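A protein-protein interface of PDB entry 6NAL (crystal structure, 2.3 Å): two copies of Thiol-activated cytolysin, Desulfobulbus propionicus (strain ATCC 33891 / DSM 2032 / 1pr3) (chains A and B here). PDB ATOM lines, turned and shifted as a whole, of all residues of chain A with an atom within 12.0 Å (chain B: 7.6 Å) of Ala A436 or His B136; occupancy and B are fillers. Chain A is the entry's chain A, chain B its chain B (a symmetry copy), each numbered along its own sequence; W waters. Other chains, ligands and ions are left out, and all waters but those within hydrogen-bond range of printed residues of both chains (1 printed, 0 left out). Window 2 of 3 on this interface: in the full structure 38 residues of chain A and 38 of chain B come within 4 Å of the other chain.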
ATOM      1  N   ARG A 379      13.985  14.098 -45.170  1.00  0.00           N
ATOM      2  CA  ARG A 379      12.597  13.909 -45.532  1.00  0.00           C
ATOM      3  C   ARG A 379      11.942  15.257 -45.709  1.00  0.00           C
ATOM      4  O   ARG A 379      12.315  16.249 -45.062  1.00  0.00           O
ATOM      5  CB  ARG A 379      11.850  13.085 -44.508  1.00  0.00           C
ATOM      6  CG  ARG A 379      11.929  13.641 -43.160  1.00  0.00           C
ATOM      7  CD  ARG A 379      11.451  12.626 -42.160  1.00  0.00           C
ATOM      8  NE  ARG A 379      11.271  13.319 -40.895  1.00  0.00           N
ATOM      9  CZ  ARG A 379      11.236  12.701 -39.728  1.00  0.00           C
ATOM     10  NH1 ARG A 379      11.324  11.373 -39.693  1.00  0.00           N
ATOM     11  NH2 ARG A 379      11.100  13.407 -38.615  1.00  0.00           N
ATOM     12  N   GLY A 431      16.703  16.993 -41.960  1.00  0.00           N
ATOM     13  CA  GLY A 431      17.864  16.223 -42.319  1.00  0.00           C
ATOM     14  C   GLY A 431      18.296  15.451 -41.108  1.00  0.00           C
ATOM     15  O   GLY A 431      18.350  16.019 -40.017  1.00  0.00           O
ATOM     16  N   CYS A 432      18.550  14.155 -41.270  1.00  0.00           N
ATOM     17  CA  CYS A 432      19.033  13.329 -40.166  1.00  0.00           C
ATOM     18  C   CYS A 432      20.515  13.598 -39.913  1.00  0.00           C
ATOM     19  O   CYS A 432      21.352  13.352 -40.794  1.00  0.00           O
ATOM     20  CB  CYS A 432      18.823  11.856 -40.473  1.00  0.00           C
ATOM     21  SG  CYS A 432      19.467  10.793 -39.150  1.00  0.00           S
ATOM     22  N   THR A 433      20.836  14.080 -38.704  1.00  0.00           N
ATOM     23  CA  THR A 433      22.215  14.379 -38.350  1.00  0.00           C
ATOM     24  C   THR A 433      23.024  13.141 -38.003  1.00  0.00           C
ATOM     25  O   THR A 433      24.253  13.208 -37.961  1.00  0.00           O
ATOM     26  CB  THR A 433      22.309  15.312 -37.142  1.00  0.00           C
ATOM     27  OG1 THR A 433      21.881  14.603 -35.967  1.00  0.00           O
ATOM     28  CG2 THR A 433      21.499  16.573 -37.330  1.00  0.00           C
ATOM     29  N   GLY A 434      22.379  12.042 -37.687  1.00  0.00           N
ATOM     30  CA  GLY A 434      23.106  10.880 -37.202  1.00  0.00           C
ATOM     31  C   GLY A 434      23.473  10.864 -35.726  1.00  0.00           C
ATOM     32  O   GLY A 434      24.025   9.859 -35.275  1.00  0.00           O
ATOM     33  N   LEU A 435      23.156  11.910 -34.958  1.00  0.00           N
ATOM     34  CA  LEU A 435      23.478  11.991 -33.534  1.00  0.00           C
ATOM     35  C   LEU A 435      22.227  11.979 -32.663  1.00  0.00           C
ATOM     36  O   LEU A 435      21.314  12.785 -32.867  1.00  0.00           O
ATOM     37  CB  LEU A 435      24.267  13.270 -33.255  1.00  0.00           C
ATOM     38  CG  LEU A 435      25.331  13.682 -34.279  1.00  0.00           C
ATOM     39  CD1 LEU A 435      25.937  15.041 -33.909  1.00  0.00           C
ATOM     40  CD2 LEU A 435      26.455  12.643 -34.432  1.00  0.00           C
ATOM     41  N   ALA A 436      22.249  11.167 -31.610  1.00  0.00           N
ATOM     42  CA  ALA A 436      21.024  10.753 -30.930  1.00  0.00           C
ATOM     43  C   ALA A 436      20.293  11.904 -30.248  1.00  0.00           C
ATOM     44  O   ALA A 436      19.054  11.897 -30.170  1.00  0.00           O
ATOM     45  CB  ALA A 436      21.368   9.672 -29.911  1.00  0.00           C
ATOM     46  N   TRP A 437      21.021  12.876 -29.715  1.00  0.00           N
ATOM     47  CA  TRP A 437      20.368  13.972 -29.009  1.00  0.00           C
ATOM     48  C   TRP A 437      19.777  15.029 -29.958  1.00  0.00           C
ATOM     49  O   TRP A 437      19.119  15.971 -29.498  1.00  0.00           O
ATOM     50  CB  TRP A 437      21.363  14.619 -28.044  1.00  0.00           C
ATOM     51  CG  TRP A 437      22.501  15.252 -28.782  1.00  0.00           C
ATOM     52  CD1 TRP A 437      22.548  16.528 -29.284  1.00  0.00           C
ATOM     53  CD2 TRP A 437      23.742  14.639 -29.129  1.00  0.00           C
ATOM     54  NE1 TRP A 437      23.751  16.745 -29.924  1.00  0.00           N
ATOM     55  CE2 TRP A 437      24.503  15.601 -29.836  1.00  0.00           C
ATOM     56  CE3 TRP A 437      24.295  13.371 -28.906  1.00  0.00           C
ATOM     57  CZ2 TRP A 437      25.786  15.331 -30.319  1.00  0.00           C
ATOM     58  CZ3 TRP A 437      25.576  13.105 -29.397  1.00  0.00           C
ATOM     59  CH2 TRP A 437      26.301  14.079 -30.095  1.00  0.00           C
ATOM     60  N   GLU A 438      19.979  14.903 -31.266  1.00  0.00           N
ATOM     61  CA  GLU A 438      19.384  15.832 -32.229  1.00  0.00           C
ATOM     62  C   GLU A 438      19.274  15.120 -33.569  1.00  0.00           C
ATOM     63  O   GLU A 438      19.881  15.548 -34.554  1.00  0.00           O
ATOM     64  CB  GLU A 438      20.186  17.140 -32.351  1.00  0.00           C
ATOM     65  CG  GLU A 438      21.655  17.016 -32.699  1.00  0.00           C
ATOM     66  CD  GLU A 438      22.425  18.357 -32.586  1.00  0.00           C
ATOM     67  OE1 GLU A 438      22.044  19.310 -33.315  1.00  0.00           O
ATOM     68  OE2 GLU A 438      23.403  18.445 -31.783  1.00  0.00           O
ATOM     69  N   TRP A 439      18.500  14.032 -33.593  1.00  0.00           N
ATOM     70  CA  TRP A 439      18.498  13.109 -34.719  1.00  0.00           C
ATOM     71  C   TRP A 439      17.983  13.757 -35.996  1.00  0.00           C
ATOM     72  O   TRP A 439      18.528  13.529 -37.080  1.00  0.00           O
ATOM     73  CB  TRP A 439      17.621  11.918 -34.347  1.00  0.00           C
ATOM     74  CG  TRP A 439      17.665  10.824 -35.297  1.00  0.00           C
ATOM     75  CD1 TRP A 439      16.685  10.436 -36.173  1.00  0.00           C
ATOM     76  CD2 TRP A 439      18.757   9.937 -35.490  1.00  0.00           C
ATOM     77  NE1 TRP A 439      17.130   9.362 -36.913  1.00  0.00           N
ATOM     78  CE2 TRP A 439      18.382   9.014 -36.481  1.00  0.00           C
ATOM     79  CE3 TRP A 439      20.022   9.832 -34.916  1.00  0.00           C
ATOM     80  CZ2 TRP A 439      19.221   8.012 -36.904  1.00  0.00           C
ATOM     81  CZ3 TRP A 439      20.832   8.847 -35.326  1.00  0.00           C
ATOM     82  CH2 TRP A 439      20.440   7.947 -36.321  1.00  0.00           C
ATOM     83  N   TRP A 440      16.871  14.476 -35.912  1.00  0.00           N
ATOM     84  CA  TRP A 440      16.304  15.143 -37.079  1.00  0.00           C
ATOM     85  C   TRP A 440      16.451  16.613 -36.810  1.00  0.00           C
ATOM     86  O   TRP A 440      16.075  17.072 -35.734  1.00  0.00           O
ATOM     87  CB  TRP A 440      14.824  14.810 -37.339  1.00  0.00           C
ATOM     88  CG  TRP A 440      14.609  13.397 -37.915  1.00  0.00           C
ATOM     89  CD1 TRP A 440      14.120  12.322 -37.240  1.00  0.00           C
ATOM     90  CD2 TRP A 440      14.900  12.922 -39.254  1.00  0.00           C
ATOM     91  NE1 TRP A 440      14.079  11.213 -38.063  1.00  0.00           N
ATOM     92  CE2 TRP A 440      14.560  11.545 -39.293  1.00  0.00           C
ATOM     93  CE3 TRP A 440      15.439  13.508 -40.400  1.00  0.00           C
ATOM     94  CZ2 TRP A 440      14.697  10.763 -40.432  1.00  0.00           C
ATOM     95  CZ3 TRP A 440      15.574  12.715 -41.560  1.00  0.00           C
ATOM     96  CH2 TRP A 440      15.204  11.356 -41.555  1.00  0.00           C
ATOM     97  N   ARG A 441      17.037  17.330 -37.755  1.00  0.00           N
ATOM     98  CA  ARG A 441      17.187  18.766 -37.666  1.00  0.00           C
ATOM     99  C   ARG A 441      16.299  19.356 -38.741  1.00  0.00           C
ATOM    100  O   ARG A 441      16.258  18.855 -39.863  1.00  0.00           O
ATOM    101  CB  ARG A 441      18.643  19.182 -37.860  1.00  0.00           C
ATOM    102  CG  ARG A 441      18.971  20.517 -37.219  1.00  0.00           C
ATOM    103  CD  ARG A 441      19.408  20.416 -35.732  1.00  0.00           C
ATOM    104  NE  ARG A 441      20.784  19.937 -35.543  1.00  0.00           N
ATOM    105  CZ  ARG A 441      21.882  20.622 -35.875  1.00  0.00           C
ATOM    106  NH1 ARG A 441      21.780  21.826 -36.412  1.00  0.00           N
ATOM    107  NH2 ARG A 441      23.092  20.115 -35.678  1.00  0.00           N
ATOM    108  N   THR A 463      25.725  16.602 -42.685  1.00  0.00           N
ATOM    109  CA  THR A 463      24.902  16.264 -41.520  1.00  0.00           C
ATOM    110  C   THR A 463      24.839  17.403 -40.509  1.00  0.00           C
ATOM    111  O   THR A 463      23.787  17.679 -39.935  1.00  0.00           O
ATOM    112  CB  THR A 463      25.475  15.030 -40.811  1.00  0.00           C
ATOM    113  OG1 THR A 463      26.895  15.185 -40.756  1.00  0.00           O
ATOM    114  CG2 THR A 463      25.148  13.700 -41.503  1.00  0.00           C
ATOM    115  N   LEU A 464      25.974  18.026 -40.211  1.00  0.00           N
ATOM    116  CA  LEU A 464      26.007  19.075 -39.195  1.00  0.00           C
ATOM    117  C   LEU A 464      25.978  20.478 -39.781  1.00  0.00           C
ATOM    118  O   LEU A 464      25.958  21.443 -39.024  1.00  0.00           O
ATOM    119  CB  LEU A 464      27.241  18.898 -38.309  1.00  0.00           C
ATOM    120  CG  LEU A 464      27.190  17.604 -37.484  1.00  0.00           C
ATOM    121  CD1 LEU A 464      27.812  16.402 -38.189  1.00  0.00           C
ATOM    122  CD2 LEU A 464      27.879  17.761 -36.118  1.00  0.00           C
ATOM    123  N   GLN A 466      23.538  21.974 -42.627  1.00  0.00           N
ATOM    124  CA  GLN A 466      22.477  21.657 -43.561  1.00  0.00           C
ATOM    125  C   GLN A 466      21.957  22.951 -44.154  1.00  0.00           C
ATOM    126  O   GLN A 466      21.557  23.852 -43.418  1.00  0.00           O
ATOM    127  CB  GLN A 466      21.327  20.918 -42.876  1.00  0.00           C
ATOM    128  CG  GLN A 466      21.639  19.530 -42.371  1.00  0.00           C
ATOM    129  CD  GLN A 466      20.407  18.868 -41.716  1.00  0.00           C
ATOM    130  OE1 GLN A 466      19.234  19.235 -41.930  1.00  0.00           O
ATOM    131  NE2 GLN A 466      20.684  17.897 -40.913  1.00  0.00           N
ATOM    132  N   LEU B 104      12.133   6.080 -29.408  1.00  0.00           N
ATOM    133  CA  LEU B 104      12.791   7.326 -29.103  1.00  0.00           C
ATOM    134  C   LEU B 104      13.601   7.798 -30.303  1.00  0.00           C
ATOM    135  O   LEU B 104      14.170   6.982 -31.042  1.00  0.00           O
ATOM    136  CB  LEU B 104      13.693   7.151 -27.910  1.00  0.00           C
ATOM    137  CG  LEU B 104      12.922   7.246 -26.608  1.00  0.00           C
ATOM    138  CD1 LEU B 104      13.729   6.524 -25.517  1.00  0.00           C
ATOM    139  CD2 LEU B 104      12.690   8.702 -26.280  1.00  0.00           C
ATOM    140  N   PRO B 105      13.661   9.114 -30.518  1.00  0.00           N
ATOM    141  CA  PRO B 105      14.431   9.635 -31.659  1.00  0.00           C
ATOM    142  C   PRO B 105      15.909   9.315 -31.463  1.00  0.00           C
ATOM    143  O   PRO B 105      16.525   9.698 -30.460  1.00  0.00           O
ATOM    144  CB  PRO B 105      14.149  11.140 -31.620  1.00  0.00           C
ATOM    145  CG  PRO B 105      14.074  11.406 -30.090  1.00  0.00           C
ATOM    146  CD  PRO B 105      13.371  10.163 -29.518  1.00  0.00           C
ATOM    147  N   GLY B 106      16.468   8.577 -32.416  1.00  0.00           N
ATOM    148  CA  GLY B 106      17.856   8.213 -32.390  1.00  0.00           C
ATOM    149  C   GLY B 106      18.102   6.924 -31.656  1.00  0.00           C
ATOM    150  O   GLY B 106      19.095   6.238 -31.924  1.00  0.00           O
ATOM    151  N   ALA B 107      17.181   6.553 -30.783  1.00  0.00           N
ATOM    152  CA  ALA B 107      17.276   5.274 -30.106  1.00  0.00           C
ATOM    153  C   ALA B 107      16.964   4.127 -31.054  1.00  0.00           C
ATOM    154  O   ALA B 107      16.226   4.270 -32.034  1.00  0.00           O
ATOM    155  CB  ALA B 107      16.312   5.206 -28.921  1.00  0.00           C
ATOM    156  N   SER B 130      14.580   6.022 -17.975  1.00  0.00           N
ATOM    157  CA  SER B 130      15.738   6.221 -17.104  1.00  0.00           C
ATOM    158  C   SER B 130      16.967   5.516 -17.647  1.00  0.00           C
ATOM    159  O   SER B 130      18.085   5.935 -17.339  1.00  0.00           O
ATOM    160  CB  SER B 130      15.465   5.739 -15.690  1.00  0.00           C
ATOM    161  OG  SER B 130      15.218   4.354 -15.701  1.00  0.00           O
ATOM    162  N   LYS B 131      16.785   4.492 -18.491  1.00  0.00           N
ATOM    163  CA  LYS B 131      17.925   3.815 -19.105  1.00  0.00           C
ATOM    164  C   LYS B 131      18.521   4.610 -20.267  1.00  0.00           C
ATOM    165  O   LYS B 131      19.749   4.690 -20.408  1.00  0.00           O
ATOM    166  CB  LYS B 131      17.529   2.410 -19.576  1.00  0.00           C
ATOM    167  CG  LYS B 131      17.389   1.337 -18.446  1.00  0.00           C
ATOM    168  CD  LYS B 131      18.255   1.584 -17.185  1.00  0.00           C
ATOM    169  CE  LYS B 131      19.780   1.965 -17.514  1.00  0.00           C
ATOM    170  NZ  LYS B 131      20.730   1.909 -16.486  1.00  0.00           N
ATOM    171  N   TRP B 132      17.676   5.181 -21.119  1.00  0.00           N
ATOM    172  CA  TRP B 132      18.173   6.014 -22.206  1.00  0.00           C
ATOM    173  C   TRP B 132      18.799   7.301 -21.694  1.00  0.00           C
ATOM    174  O   TRP B 132      19.753   7.787 -22.304  1.00  0.00           O
ATOM    175  CB  TRP B 132      17.018   6.308 -23.136  1.00  0.00           C
ATOM    176  CG  TRP B 132      17.194   7.380 -24.163  1.00  0.00           C
ATOM    177  CD1 TRP B 132      16.800   8.695 -24.075  1.00  0.00           C
ATOM    178  CD2 TRP B 132      17.739   7.213 -25.468  1.00  0.00           C
ATOM    179  NE1 TRP B 132      17.085   9.354 -25.249  1.00  0.00           N
ATOM    180  CE2 TRP B 132      17.663   8.470 -26.120  1.00  0.00           C
ATOM    181  CE3 TRP B 132      18.303   6.126 -26.148  1.00  0.00           C
ATOM    182  CZ2 TRP B 132      18.126   8.669 -27.424  1.00  0.00           C
ATOM    183  CZ3 TRP B 132      18.778   6.325 -27.439  1.00  0.00           C
ATOM    184  CH2 TRP B 132      18.670   7.587 -28.072  1.00  0.00           C
ATOM    185  N   PHE B 133      18.293   7.857 -20.580  1.00  0.00           N
ATOM    186  CA  PHE B 133      18.882   9.075 -20.014  1.00  0.00           C
ATOM    187  C   PHE B 133      20.246   8.789 -19.376  1.00  0.00           C
ATOM    188  O   PHE B 133      21.175   9.607 -19.481  1.00  0.00           O
ATOM    189  CB  PHE B 133      17.940   9.712 -18.979  1.00  0.00           C
ATOM    190  CG  PHE B 133      16.768  10.465 -19.584  1.00  0.00           C
ATOM    191  CD1 PHE B 133      16.932  11.294 -20.696  1.00  0.00           C
ATOM    192  CD2 PHE B 133      15.493  10.339 -19.036  1.00  0.00           C
ATOM    193  CE1 PHE B 133      15.844  11.969 -21.255  1.00  0.00           C
ATOM    194  CE2 PHE B 133      14.406  11.021 -19.588  1.00  0.00           C
ATOM    195  CZ  PHE B 133      14.590  11.847 -20.697  1.00  0.00           C
ATOM    196  N   ASP B 134      20.382   7.637 -18.705  1.00  0.00           N
ATOM    197  CA  ASP B 134      21.630   7.296 -18.029  1.00  0.00           C
ATOM    198  C   ASP B 134      22.738   7.017 -19.029  1.00  0.00           C
ATOM    199  O   ASP B 134      23.908   7.328 -18.771  1.00  0.00           O
ATOM    200  CB  ASP B 134      21.429   6.083 -17.123  1.00  0.00           C
ATOM    201  CG  ASP B 134      20.587   6.396 -15.912  1.00  0.00           C
ATOM    202  OD1 ASP B 134      19.809   5.508 -15.486  1.00  0.00           O
ATOM    203  OD2 ASP B 134      20.700   7.531 -15.391  1.00  0.00           O
ATOM    204  N   SER B 135      22.396   6.439 -20.179  1.00  0.00           N
ATOM    205  CA  SER B 135      23.392   6.177 -21.209  1.00  0.00           C
ATOM    206  C   SER B 135      23.607   7.387 -22.117  1.00  0.00           C
ATOM    207  O   SER B 135      23.911   7.227 -23.310  1.00  0.00           O
ATOM    208  CB  SER B 135      22.973   4.957 -22.035  1.00  0.00           C
ATOM    209  OG  SER B 135      21.891   5.268 -22.908  1.00  0.00           O
ATOM    210  N   HIS B 136      23.444   8.596 -21.570  1.00  0.00           N
ATOM    211  CA  HIS B 136      23.622   9.829 -22.336  1.00  0.00           C
ATOM    212  C   HIS B 136      24.132  10.933 -21.420  1.00  0.00           C
ATOM    213  O   HIS B 136      23.519  11.234 -20.389  1.00  0.00           O
ATOM    214  CB  HIS B 136      22.309  10.251 -23.015  1.00  0.00           C
ATOM    215  CG  HIS B 136      21.993   9.452 -24.239  1.00  0.00           C
ATOM    216  ND1 HIS B 136      21.697   8.108 -24.189  1.00  0.00           N
ATOM    217  CD2 HIS B 136      21.957   9.796 -25.549  1.00  0.00           C
ATOM    218  CE1 HIS B 136      21.480   7.657 -25.413  1.00  0.00           C
ATOM    219  NE2 HIS B 136      21.637   8.661 -26.258  1.00  0.00           N
ATOM    220  N   GLY B 137      25.265  11.527 -21.786  1.00  0.00           N
ATOM    221  CA  GLY B 137      25.678  12.745 -21.123  1.00  0.00           C
ATOM    222  C   GLY B 137      24.743  13.905 -21.379  1.00  0.00           C
ATOM    223  O   GLY B 137      24.861  14.945 -20.719  1.00  0.00           O
ATOM    224  N   GLY B 138      23.818  13.749 -22.322  1.00  0.00           N
ATOM    225  CA  GLY B 138      22.849  14.780 -22.598  1.00  0.00           C
ATOM    226  C   GLY B 138      21.754  14.807 -21.556  1.00  0.00           C
ATOM    227  O   GLY B 138      21.083  13.802 -21.297  1.00  0.00           O
ATOM    228  N   GLU B 139      21.600  15.969 -20.933  1.00  0.00           N
ATOM    229  CA  GLU B 139      20.379  16.259 -20.207  1.00  0.00           C
ATOM    230  C   GLU B 139      19.178  16.419 -21.144  1.00  0.00           C
ATOM    231  O   GLU B 139      18.065  16.054 -20.767  1.00  0.00           O
ATOM    232  CB  GLU B 139      20.563  17.533 -19.388  1.00  0.00           C
ATOM    233  CG  GLU B 139      19.257  18.196 -18.987  1.00  0.00           C
ATOM    234  CD  GLU B 139      19.417  19.113 -17.777  1.00  0.00           C
ATOM    235  OE1 GLU B 139      20.302  20.002 -17.837  1.00  0.00           O
ATOM    236  OE2 GLU B 139      18.660  18.943 -16.781  1.00  0.00           O
ATOM    237  N   TRP B 140      19.364  16.979 -22.349  1.00  0.00           N
ATOM    238  CA  TRP B 140      18.240  17.273 -23.246  1.00  0.00           C
ATOM    239  C   TRP B 140      18.422  16.727 -24.668  1.00  0.00           C
ATOM    240  O   TRP B 140      19.529  16.597 -25.169  1.00  0.00           O
ATOM    241  CB  TRP B 140      17.991  18.781 -23.394  1.00  0.00           C
ATOM    242  CG  TRP B 140      17.677  19.511 -22.140  1.00  0.00           C
ATOM    243  CD1 TRP B 140      16.565  19.389 -21.347  1.00  0.00           C
ATOM    244  CD2 TRP B 140      18.424  20.583 -21.620  1.00  0.00           C
ATOM    245  NE1 TRP B 140      16.620  20.300 -20.321  1.00  0.00           N
ATOM    246  CE2 TRP B 140      17.757  21.052 -20.469  1.00  0.00           C
ATOM    247  CE3 TRP B 140      19.619  21.193 -22.009  1.00  0.00           C
ATOM    248  CZ2 TRP B 140      18.272  22.087 -19.665  1.00  0.00           C
ATOM    249  CZ3 TRP B 140      20.129  22.247 -21.224  1.00  0.00           C
ATOM    250  CH2 TRP B 140      19.441  22.687 -20.067  1.00  0.00           C
ATOM    251  N   SER B 141      17.321  16.343 -25.299  1.00  0.00           N
ATOM    252  CA  SER B 141      17.321  15.878 -26.683  1.00  0.00           C
ATOM    253  C   SER B 141      16.220  16.598 -27.473  1.00  0.00           C
ATOM    254  O   SER B 141      15.268  17.155 -26.915  1.00  0.00           O
ATOM    255  CB  SER B 141      17.128  14.356 -26.715  1.00  0.00           C
ATOM    256  OG  SER B 141      15.742  14.034 -26.683  1.00  0.00           O
ATOM    257  N   LEU B 142      16.378  16.614 -28.759  1.00  0.00           N
ATOM    258  CA  LEU B 142      15.400  17.278 -29.605  1.00  0.00           C
ATOM    259  C   LEU B 142      14.170  16.384 -29.791  1.00  0.00           C
ATOM    260  O   LEU B 142      14.305  15.171 -29.927  1.00  0.00           O
ATOM    261  CB  LEU B 142      15.987  17.566 -30.975  1.00  0.00           C
ATOM    262  CG  LEU B 142      16.699  18.878 -31.331  1.00  0.00           C
ATOM    263  CD1 LEU B 142      16.916  18.953 -32.896  1.00  0.00           C
ATOM    264  CD2 LEU B 142      16.023  20.141 -30.862  1.00  0.00           C
ATOM    265  N   ARG B 327      15.001  14.441 -18.219  1.00  0.00           N
ATOM    266  CA  ARG B 327      14.664  13.523 -17.134  1.00  0.00           C
ATOM    267  C   ARG B 327      13.599  14.108 -16.232  1.00  0.00           C
ATOM    268  O   ARG B 327      12.668  13.406 -15.815  1.00  0.00           O
ATOM    269  CB  ARG B 327      15.928  13.225 -16.312  1.00  0.00           C
ATOM    270  CG  ARG B 327      15.988  11.860 -15.674  1.00  0.00           C
ATOM    271  CD  ARG B 327      17.123  11.738 -14.648  1.00  0.00           C
ATOM    272  NE  ARG B 327      17.041  10.422 -14.035  1.00  0.00           N
ATOM    273  CZ  ARG B 327      17.615   9.336 -14.534  1.00  0.00           C
ATOM    274  NH1 ARG B 327      18.349   9.407 -15.636  1.00  0.00           N
ATOM    275  NH2 ARG B 327      17.468   8.176 -13.925  1.00  0.00           N
HETATM  276  O   HOH W   1      16.369  13.837 -31.461  1.00  0.00           O
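No position is printed for both chains.
Among the printed residues, pairs that only touch across the chains: Trp A437 with Ser B141, Trp A440 with Leu B142, Trp A439 with Gly B106, Glu A438 with Leu B142, Ala A436 with His B136, Ala A436 with Trp B132 and Trp A437 with Trp B140.
Ala A436 touches just these residues of chain B: Pro B105, Trp B132 and His B136. His B136 touches one residue of chain A. Gly B106 touches one residue of chain A. Of chain A, only Ala A436 comes within 4 Å of Trp B132. No residue of chain A comes within 4 Å of Ser B135. No residue of chain A comes within 4 Å of Gly B138. Of the printed residues of chain A, Ser B141 touches Trp A437 (3.3 Å). Of the printed residues of chain B, Trp A439 touches Gly B106 (3.7 Å). Printed residues of chain B within 4 Å of Glu A438: Leu B142. Of the printed residues of chain A, Leu B142 touches Trp A437 (2.9 Å), Glu A438 (3.8 Å) and Trp A440 (3.5 Å). Of the printed residues of chain B, Trp A437 touches Trp B140 (3.9 Å), Ser B141 (3.3 Å) and Leu B142 (2.9 Å). Leu A464 touches none of the printed residues of chain B. The nearest residue of chain A that does not touch His B136 is Trp A437 (5.3 Å).
The side-chain sulfur (SG) of Cys A432 lies close to the indole nitrogen (NE1) of Trp A439. The side-chain carboxylate (OE2) of Glu A438 sits at hydrogen-bond distance from the indole nitrogen (NE1) of Trp A437. NE of Arg A441 lies within salt-bridge range of OE1 of Glu A438 (2.6 Å). The backbone carbonyl oxygen (O) of Trp B132 is in hydrogen-bond range of the side-chain hydroxyl (OG) of Ser B135, 3.4 Å away. The backbone carbonyl oxygen (O) of Trp B132 lies within hydrogen-bond range of a ring nitrogen (ND1) of His B136 (2.7 Å). The side-chain hydroxyl of Ser B135 sits close to a ring nitrogen (ND1) of His B136 (3.1 Å).
O of Trp A437 is in hydrogen-bond range of N of Leu B142 (2.9 Å). The backbone carbonyl oxygen of Pro B105 sits close to the backbone carbonyl oxygen of Ala A436 (3.4 Å).
Hydrophobic or aromatic side chains of chain A within 4 Å of the printed part of chain B: Ala A436, Trp A437 and Trp A439. Of the 18 printed residues of chain B, 7 touch a printed residue of chain A. Hydrophobic or aromatic side chains of chain B that line the printed part of chain A: Trp B132, His B136 and Leu B142.
Water W1 bridges the backbone carbonyl oxygen (O) of Leu B142 (2.9 Å) and the backbone NH (N) of Trp A439 (3.0 Å).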
